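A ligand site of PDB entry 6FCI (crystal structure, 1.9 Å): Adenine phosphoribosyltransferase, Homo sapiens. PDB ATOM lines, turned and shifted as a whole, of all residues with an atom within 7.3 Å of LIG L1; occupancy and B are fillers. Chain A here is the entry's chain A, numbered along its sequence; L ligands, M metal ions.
Val 23 touches LIG L1.
Phe 25 touches LIG L1 (CE1 to C4, 3.3 Å).
Leu 128 touches LIG L1 (CD2 to C2, 3.7 Å).
Ala 130 touches LIG L1.
Leu 158 touches LIG L1.
Hydrophobic or aromatic side chains that line LIG L1: Val 23, Phe 25, Tyr 104, Leu 128, Ala 130 and Leu 158.
Ten residues have an atom within 4 Å of LIG L1: Val 23, Val 24, Phe 25, Arg 26, Arg 66, Glu 103, Tyr 104, Leu 128, Ala 130 and Leu 158.
The nearest printed residue that does not touch LIG L1 is Leu 102 (4.7 Å).
N1 of LIG L1 sits at hydrogen-bond distance from O4 of LG2 L2 (3.1 Å).
The side-chain carboxylate (OD1) of Asp 127 sits close to an oxygen (O2) of LG2 L2, at 2.7 Å.
An oxygen (O6) of LG2 L2 is in hydrogen-bond range of the backbone NH (N) of Thr 131 (2.9 Å).
N of Arg 26 sits at hydrogen-bond distance from N4 of LIG L1 (2.9 Å).
An oxygen (O6) of LG2 L2 sits at hydrogen-bond distance from the side-chain hydroxyl (OG1) of Thr 131, at 2.5 Å.
O7 of LG2 L2 lies within hydrogen-bond range of N of Thr 134 (2.9 Å).
The backbone NH of Arg 66 lies close to an oxygen (O14) of LG2 L2 (3.1 Å).
N3 of LIG L1 is in hydrogen-bond range of O of Val 24, at 3.1 Å.
O7 of LG2 L2 is in hydrogen-bond range of OG1 of Thr 134, at 2.6 Å.
O6 of LG2 L2 lies within hydrogen-bond range of N of Glu 103 (2.8 Å).
OH of Tyr 104 is in hydrogen-bond range of N1 of LIG L1 (3.4 Å).
N of Ala 130 is in hydrogen-bond range of O8 of LG2 L2, 2.7 Å away.
The guanidinium group of Arg 66 lies within salt-bridge range of an oxygen (O13) of LG2 L2, 2.7 Å away.
NH1 of Arg 66 sits at hydrogen-bond distance from N5 of LIG L1 (2.9 Å).
N2 of LIG L1 sits at hydrogen-bond distance from OE1 of Glu 103, at 2.6 Å.
OH of Tyr 104 is in hydrogen-bond range of O10 of LG2 L2 (2.5 Å).
The backbone NH (N) of Leu 158 lies within hydrogen-bond range of the backbone carbonyl oxygen (O) of Leu 129, at 3.0 Å.
O of Phe 15 is in hydrogen-bond range of N of Phe 25 (2.7 Å).
The side-chain hydroxyl (OH) of Tyr 104 lies within hydrogen-bond range of the guanidinium group (NH2) of Arg 66 (2.9 Å).
The guanidinium group (NH1) of Arg 66 is in salt-bridge range of the side-chain carboxylate (OD2) of Asp 127 (2.8 Å).
The backbone NH of Phe 18 sits at hydrogen-bond distance from the backbone carbonyl oxygen of Val 23 (3.4 Å).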
ATOM      1  N   PHE A  15       3.912  13.643  13.249  1.00  0.00           N
ATOM      2  CA  PHE A  15       3.427  12.707  14.256  1.00  0.00           C
ATOM      3  C   PHE A  15       3.904  13.161  15.623  1.00  0.00           C
ATOM      4  O   PHE A  15       5.102  13.297  15.862  1.00  0.00           O
ATOM      5  CB  PHE A  15       4.000  11.312  13.990  1.00  0.00           C
ATOM      6  CG  PHE A  15       3.525  10.696  12.715  1.00  0.00           C
ATOM      7  CD1 PHE A  15       4.152  11.009  11.521  1.00  0.00           C
ATOM      8  CD2 PHE A  15       2.449   9.842  12.703  1.00  0.00           C
ATOM      9  CE1 PHE A  15       3.721  10.451  10.336  1.00  0.00           C
ATOM     10  CE2 PHE A  15       2.006   9.276  11.523  1.00  0.00           C
ATOM     11  CZ  PHE A  15       2.646   9.585  10.333  1.00  0.00           C
ATOM     12  N   PHE A  18       6.593  10.879  18.879  1.00  0.00           N
ATOM     13  CA  PHE A  18       7.424   9.832  18.304  1.00  0.00           C
ATOM     14  C   PHE A  18       8.835  10.357  18.049  1.00  0.00           C
ATOM     15  O   PHE A  18       8.998  11.445  17.504  1.00  0.00           O
ATOM     16  CB  PHE A  18       6.818   9.339  16.988  1.00  0.00           C
ATOM     17  CG  PHE A  18       7.547   8.181  16.383  1.00  0.00           C
ATOM     18  CD1 PHE A  18       7.226   6.887  16.740  1.00  0.00           C
ATOM     19  CD2 PHE A  18       8.601   8.398  15.511  1.00  0.00           C
ATOM     20  CE1 PHE A  18       7.931   5.810  16.216  1.00  0.00           C
ATOM     21  CE2 PHE A  18       9.310   7.330  14.988  1.00  0.00           C
ATOM     22  CZ  PHE A  18       8.976   6.041  15.340  1.00  0.00           C
ATOM     23  N   PRO A  19       9.859   9.597  18.428  1.00  0.00           N
ATOM     24  CA  PRO A  19       9.706   8.250  18.989  1.00  0.00           C
ATOM     25  C   PRO A  19       9.608   8.251  20.512  1.00  0.00           C
ATOM     26  O   PRO A  19       9.674   7.206  21.151  1.00  0.00           O
ATOM     27  CB  PRO A  19      11.003   7.563  18.568  1.00  0.00           C
ATOM     28  CG  PRO A  19      12.002   8.661  18.469  1.00  0.00           C
ATOM     29  CD  PRO A  19      11.247   9.898  18.054  1.00  0.00           C
ATOM     30  N   VAL A  23       8.339  14.833  21.447  1.00  0.00           N
ATOM     31  CA  VAL A  23       8.867  15.025  20.098  1.00  0.00           C
ATOM     32  C   VAL A  23       7.740  15.099  19.075  1.00  0.00           C
ATOM     33  O   VAL A  23       6.858  14.238  19.030  1.00  0.00           O
ATOM     34  CB  VAL A  23       9.824  13.887  19.693  1.00  0.00           C
ATOM     35  CG1 VAL A  23      10.253  14.053  18.239  1.00  0.00           C
ATOM     36  CG2 VAL A  23      11.035  13.870  20.611  1.00  0.00           C
ATOM     37  N   VAL A  24       7.779  16.140  18.254  1.00  0.00           N
ATOM     38  CA  VAL A  24       6.914  16.249  17.075  1.00  0.00           C
ATOM     39  C   VAL A  24       7.678  15.822  15.830  1.00  0.00           C
ATOM     40  O   VAL A  24       8.492  16.567  15.295  1.00  0.00           O
ATOM     41  CB  VAL A  24       6.403  17.693  16.876  1.00  0.00           C
ATOM     42  CG1 VAL A  24       5.598  17.792  15.590  1.00  0.00           C
ATOM     43  CG2 VAL A  24       5.566  18.126  18.067  1.00  0.00           C
ATOM     44  N   PHE A  25       7.402  14.600  15.379  1.00  0.00           N
ATOM     45  CA  PHE A  25       8.226  13.966  14.369  1.00  0.00           C
ATOM     46  C   PHE A  25       7.791  14.401  12.976  1.00  0.00           C
ATOM     47  O   PHE A  25       6.622  14.288  12.617  1.00  0.00           O
ATOM     48  CB  PHE A  25       8.151  12.438  14.495  1.00  0.00           C
ATOM     49  CG  PHE A  25       9.203  11.719  13.712  1.00  0.00           C
ATOM     50  CD1 PHE A  25      10.458  11.500  14.262  1.00  0.00           C
ATOM     51  CD2 PHE A  25       8.958  11.264  12.429  1.00  0.00           C
ATOM     52  CE1 PHE A  25      11.435  10.838  13.545  1.00  0.00           C
ATOM     53  CE2 PHE A  25       9.930  10.604  11.704  1.00  0.00           C
ATOM     54  CZ  PHE A  25      11.169  10.391  12.262  1.00  0.00           C
ATOM     55  N   ARG A  26       8.735  14.934  12.200  1.00  0.00           N
ATOM     56  CA  ARG A  26       8.463  15.309  10.822  1.00  0.00           C
ATOM     57  C   ARG A  26       8.820  14.174   9.867  1.00  0.00           C
ATOM     58  O   ARG A  26       9.987  13.796   9.738  1.00  0.00           O
ATOM     59  CB  ARG A  26       9.233  16.579  10.436  1.00  0.00           C
ATOM     60  CG  ARG A  26       9.127  17.697  11.452  1.00  0.00           C
ATOM     61  CD  ARG A  26       7.707  18.209  11.597  1.00  0.00           C
ATOM     62  NE  ARG A  26       7.607  19.250  12.608  1.00  0.00           N
ATOM     63  CZ  ARG A  26       6.522  19.991  12.832  1.00  0.00           C
ATOM     64  NH1 ARG A  26       5.430  19.791  12.111  1.00  0.00           N
ATOM     65  NH2 ARG A  26       6.533  20.918  13.772  1.00  0.00           N
ATOM     66  N   ASP A  27       7.806  13.616   9.224  1.00  0.00           N
ATOM     67  CA  ASP A  27       7.982  12.460   8.347  1.00  0.00           C
ATOM     68  C   ASP A  27       8.214  12.909   6.911  1.00  0.00           C
ATOM     69  O   ASP A  27       7.344  13.532   6.304  1.00  0.00           O
ATOM     70  CB  ASP A  27       6.758  11.551   8.404  1.00  0.00           C
ATOM     71  CG  ASP A  27       6.921  10.293   7.570  1.00  0.00           C
ATOM     72  OD1 ASP A  27       8.049  10.019   7.111  1.00  0.00           O
ATOM     73  OD2 ASP A  27       5.924   9.572   7.368  1.00  0.00           O
ATOM     74  N   ILE A  28       9.393  12.587   6.375  1.00  0.00           N
ATOM     75  CA  ILE A  28       9.760  12.965   5.021  1.00  0.00           C
ATOM     76  C   ILE A  28       9.247  11.976   3.974  1.00  0.00           C
ATOM     77  O   ILE A  28       9.397  12.207   2.780  1.00  0.00           O
ATOM     78  CB  ILE A  28      11.293  13.082   4.849  1.00  0.00           C
ATOM     79  CG1 ILE A  28      11.956  11.731   5.162  1.00  0.00           C
ATOM     80  CG2 ILE A  28      11.840  14.211   5.705  1.00  0.00           C
ATOM     81  CD1 ILE A  28      13.441  11.697   4.885  1.00  0.00           C
ATOM     82  N   ARG A  66      18.917   8.874   6.827  1.00  0.00           N
ATOM     83  CA  ARG A  66      17.933   9.625   6.051  1.00  0.00           C
ATOM     84  C   ARG A  66      18.597  10.655   5.146  1.00  0.00           C
ATOM     85  O   ARG A  66      18.051  11.018   4.112  1.00  0.00           O
ATOM     86  CB  ARG A  66      16.915  10.299   6.977  1.00  0.00           C
ATOM     87  CG  ARG A  66      15.842   9.350   7.469  1.00  0.00           C
ATOM     88  CD  ARG A  66      14.773  10.075   8.261  1.00  0.00           C
ATOM     89  NE  ARG A  66      15.041  10.019   9.687  1.00  0.00           N
ATOM     90  CZ  ARG A  66      14.621  10.934  10.553  1.00  0.00           C
ATOM     91  NH1 ARG A  66      13.944  11.994  10.138  1.00  0.00           N
ATOM     92  NH2 ARG A  66      14.881  10.787  11.844  1.00  0.00           N
ATOM     93  N   LEU A 102      21.464  13.724  19.571  1.00  0.00           N
ATOM     94  CA  LEU A 102      20.474  14.310  18.690  1.00  0.00           C
ATOM     95  C   LEU A 102      19.240  14.595  19.533  1.00  0.00           C
ATOM     96  O   LEU A 102      19.266  14.417  20.757  1.00  0.00           O
ATOM     97  CB  LEU A 102      20.133  13.346  17.547  1.00  0.00           C
ATOM     98  CG  LEU A 102      19.620  11.971  17.999  1.00  0.00           C
ATOM     99  CD1 LEU A 102      18.623  11.434  16.985  1.00  0.00           C
ATOM    100  CD2 LEU A 102      20.764  11.000  18.208  1.00  0.00           C
ATOM    101  N   GLU A 103      18.152  15.010  18.898  1.00  0.00           N
ATOM    102  CA  GLU A 103      16.988  15.473  19.641  1.00  0.00           C
ATOM    103  C   GLU A 103      16.471  14.432  20.633  1.00  0.00           C
ATOM    104  O   GLU A 103      16.076  14.770  21.740  1.00  0.00           O
ATOM    105  CB  GLU A 103      15.852  15.878  18.693  1.00  0.00           C
ATOM    106  CG  GLU A 103      14.655  16.470  19.441  1.00  0.00           C
ATOM    107  CD  GLU A 103      13.491  16.800  18.537  1.00  0.00           C
ATOM    108  OE1 GLU A 103      13.587  16.593  17.311  1.00  0.00           O
ATOM    109  OE2 GLU A 103      12.453  17.274  19.058  1.00  0.00           O
ATOM    110  N   TYR A 104      16.447  13.170  20.217  1.00  0.00           N
ATOM    111  CA  TYR A 104      15.781  12.133  21.010  1.00  0.00           C
ATOM    112  C   TYR A 104      16.677  10.942  21.347  1.00  0.00           C
ATOM    113  O   TYR A 104      16.197   9.835  21.565  1.00  0.00           O
ATOM    114  CB  TYR A 104      14.493  11.643  20.314  1.00  0.00           C
ATOM    115  CG  TYR A 104      14.644  11.356  18.838  1.00  0.00           C
ATOM    116  CD1 TYR A 104      15.374  10.270  18.390  1.00  0.00           C
ATOM    117  CD2 TYR A 104      13.992  12.151  17.897  1.00  0.00           C
ATOM    118  CE1 TYR A 104      15.501  10.001  17.038  1.00  0.00           C
ATOM    119  CE2 TYR A 104      14.095  11.880  16.544  1.00  0.00           C
ATOM    120  CZ  TYR A 104      14.855  10.813  16.120  1.00  0.00           C
ATOM    121  OH  TYR A 104      14.962  10.541  14.777  1.00  0.00           O
ATOM    122  N   ASP A 127      18.553  15.144   6.073  1.00  0.00           N
ATOM    123  CA  ASP A 127      17.129  15.355   5.843  1.00  0.00           C
ATOM    124  C   ASP A 127      16.584  16.464   6.746  1.00  0.00           C
ATOM    125  O   ASP A 127      15.820  17.322   6.300  1.00  0.00           O
ATOM    126  CB  ASP A 127      16.333  14.056   6.037  1.00  0.00           C
ATOM    127  CG  ASP A 127      16.260  13.613   7.480  1.00  0.00           C
ATOM    128  OD1 ASP A 127      17.297  13.609   8.167  1.00  0.00           O
ATOM    129  OD2 ASP A 127      15.156  13.218   7.920  1.00  0.00           O
ATOM    130  N   LEU A 128      16.994  16.455   8.004  1.00  0.00           N
ATOM    131  CA  LEU A 128      16.443  17.394   8.990  1.00  0.00           C
ATOM    132  C   LEU A 128      17.519  17.861   9.955  1.00  0.00           C
ATOM    133  O   LEU A 128      18.368  17.068  10.384  1.00  0.00           O
ATOM    134  CB  LEU A 128      15.275  16.731   9.743  1.00  0.00           C
ATOM    135  CG  LEU A 128      14.461  17.585  10.710  1.00  0.00           C
ATOM    136  CD1 LEU A 128      12.992  17.192  10.648  1.00  0.00           C
ATOM    137  CD2 LEU A 128      14.986  17.425  12.134  1.00  0.00           C
ATOM    138  N   LEU A 129      17.518  19.154  10.255  1.00  0.00           N
ATOM    139  CA  LEU A 129      18.287  19.698  11.372  1.00  0.00           C
ATOM    140  C   LEU A 129      17.398  19.947  12.587  1.00  0.00           C
ATOM    141  O   LEU A 129      16.380  20.626  12.502  1.00  0.00           O
ATOM    142  CB  LEU A 129      18.972  21.009  10.976  1.00  0.00           C
ATOM    143  CG  LEU A 129      19.837  21.646  12.079  1.00  0.00           C
ATOM    144  CD1 LEU A 129      21.186  20.975  12.159  1.00  0.00           C
ATOM    145  CD2 LEU A 129      19.998  23.134  11.851  1.00  0.00           C
ATOM    146  N   ALA A 130      17.792  19.393  13.732  1.00  0.00           N
ATOM    147  CA  ALA A 130      17.117  19.681  14.991  1.00  0.00           C
ATOM    148  C   ALA A 130      18.066  20.364  15.974  1.00  0.00           C
ATOM    149  O   ALA A 130      18.258  21.572  15.905  1.00  0.00           O
ATOM    150  CB  ALA A 130      16.528  18.406  15.595  1.00  0.00           C
ATOM    151  N   THR A 131      18.648  19.596  16.896  1.00  0.00           N
ATOM    152  CA  THR A 131      19.619  20.165  17.839  1.00  0.00           C
ATOM    153  C   THR A 131      20.930  20.520  17.142  1.00  0.00           C
ATOM    154  O   THR A 131      21.721  21.300  17.659  1.00  0.00           O
ATOM    155  CB  THR A 131      19.934  19.223  19.028  1.00  0.00           C
ATOM    156  OG1 THR A 131      20.636  18.062  18.557  1.00  0.00           O
ATOM    157  CG2 THR A 131      18.668  18.798  19.747  1.00  0.00           C
ATOM    158  N   THR A 134      23.941  15.982  15.231  1.00  0.00           N
ATOM    159  CA  THR A 134      24.336  15.057  14.186  1.00  0.00           C
ATOM    160  C   THR A 134      25.220  15.743  13.142  1.00  0.00           C
ATOM    161  O   THR A 134      26.260  15.213  12.754  1.00  0.00           O
ATOM    162  CB  THR A 134      23.107  14.440  13.485  1.00  0.00           C
ATOM    163  OG1 THR A 134      22.297  13.771  14.454  1.00  0.00           O
ATOM    164  CG2 THR A 134      23.545  13.447  12.408  1.00  0.00           C
ATOM    165  N   VAL A 156      14.583  20.177   6.150  1.00  0.00           N
ATOM    166  CA  VAL A 156      13.793  20.711   7.248  1.00  0.00           C
ATOM    167  C   VAL A 156      14.666  21.228   8.381  1.00  0.00           C
ATOM    168  O   VAL A 156      15.696  20.626   8.708  1.00  0.00           O
ATOM    169  CB  VAL A 156      12.825  19.660   7.808  1.00  0.00           C
ATOM    170  CG1 VAL A 156      12.070  20.201   9.014  1.00  0.00           C
ATOM    171  CG2 VAL A 156      11.857  19.198   6.728  1.00  0.00           C
ATOM    172  N   LEU A 158      14.199  22.693  12.459  1.00  0.00           N
ATOM    173  CA  LEU A 158      13.366  22.966  13.630  1.00  0.00           C
ATOM    174  C   LEU A 158      13.983  24.079  14.474  1.00  0.00           C
ATOM    175  O   LEU A 158      14.831  23.833  15.326  1.00  0.00           O
ATOM    176  CB  LEU A 158      13.199  21.694  14.477  1.00  0.00           C
ATOM    177  CG  LEU A 158      12.742  20.446  13.715  1.00  0.00           C
ATOM    178  CD1 LEU A 158      12.621  19.262  14.658  1.00  0.00           C
ATOM    179  CD2 LEU A 158      11.429  20.699  12.986  1.00  0.00           C
ATOM    180  N   LEU A 161      14.973  24.584  18.332  1.00  0.00           N
ATOM    181  CA  LEU A 161      16.042  23.784  18.917  1.00  0.00           C
ATOM    182  C   LEU A 161      17.418  24.396  18.650  1.00  0.00           C
ATOM    183  O   LEU A 161      18.437  23.902  19.134  1.00  0.00           O
ATOM    184  CB  LEU A 161      15.983  22.346  18.374  1.00  0.00           C
ATOM    185  CG  LEU A 161      14.704  21.611  18.776  1.00  0.00           C
ATOM    186  CD1 LEU A 161      14.639  20.219  18.165  1.00  0.00           C
ATOM    187  CD2 LEU A 161      14.586  21.545  20.285  1.00  0.00           C
HETATM  188  N1  LIG L   1      15.426  13.813  13.821  1.00  0.00           N
HETATM  189  C1  LIG L   1      15.667  14.527  14.941  1.00  0.00           C
HETATM  190  N2  LIG L   1      14.549  15.170  15.351  1.00  0.00           N
HETATM  191  C2  LIG L   1      13.565  14.881  14.488  1.00  0.00           C
HETATM  192  C3  LIG L   1      12.171  15.218  14.345  1.00  0.00           C
HETATM  193  N3  LIG L   1      11.576  16.046  15.275  1.00  0.00           N
HETATM  194  N4  LIG L   1      11.462  14.683  13.290  1.00  0.00           N
HETATM  195  C4  LIG L   1      12.056  13.865  12.396  1.00  0.00           C
HETATM  196  N5  LIG L   1      13.356  13.531  12.471  1.00  0.00           N
HETATM  197  C5  LIG L   1      14.102  14.021  13.512  1.00  0.00           C
HETATM  198  C1  LG2 L   2      17.802  12.065  12.743  1.00  0.00           C
HETATM  199  C2  LG2 L   2      17.697  12.890  11.471  1.00  0.00           C
HETATM  200  C3  LG2 L   2      18.935  13.759  11.535  1.00  0.00           C
HETATM  201  C4  LG2 L   2      19.165  13.971  13.026  1.00  0.00           C
HETATM  202  C5  LG2 L   2      18.704  15.376  13.431  1.00  0.00           C
HETATM  203  O1  LG2 L   2      18.599  10.920  12.466  1.00  0.00           O
HETATM  204  O2  LG2 L   2      17.675  12.055  10.308  1.00  0.00           O
HETATM  205  O3  LG2 L   2      20.052  13.055  10.959  1.00  0.00           O
HETATM  206  O4  LG2 L   2      18.427  12.940  13.697  1.00  0.00           O
HETATM  207  O5  LG2 L   2      18.714  15.541  14.847  1.00  0.00           O
HETATM  208  P1  LG2 L   2      19.764  16.543  15.576  1.00  0.00           P
HETATM  209  O6  LG2 L   2      19.165  16.759  16.942  1.00  0.00           O
HETATM  210  O7  LG2 L   2      21.067  15.783  15.606  1.00  0.00           O
HETATM  211  O8  LG2 L   2      19.770  17.767  14.703  1.00  0.00           O
HETATM  212  P2  LG2 L   2      18.452   9.544  13.308  1.00  0.00           P
HETATM  213  O9  LG2 L   2      19.582   9.491  14.300  1.00  0.00           O
HETATM  214  O10 LG2 L   2      17.024   9.426  13.800  1.00  0.00           O
HETATM  215  O11 LG2 L   2      18.756   8.356  12.245  1.00  0.00           O
HETATM  216  P3  LG2 L   2      18.077   8.114  10.796  1.00  0.00           P
HETATM  217  O12 LG2 L   2      18.484   6.695  10.501  1.00  0.00           O
HETATM  218  O13 LG2 L   2      16.587   8.289  11.012  1.00  0.00           O
HETATM  219  O14 LG2 L   2      18.701   9.137   9.886  1.00  0.00           O
HETATM  220 MG    MG M   1      19.461  10.949  10.413  1.00  0.00          MG
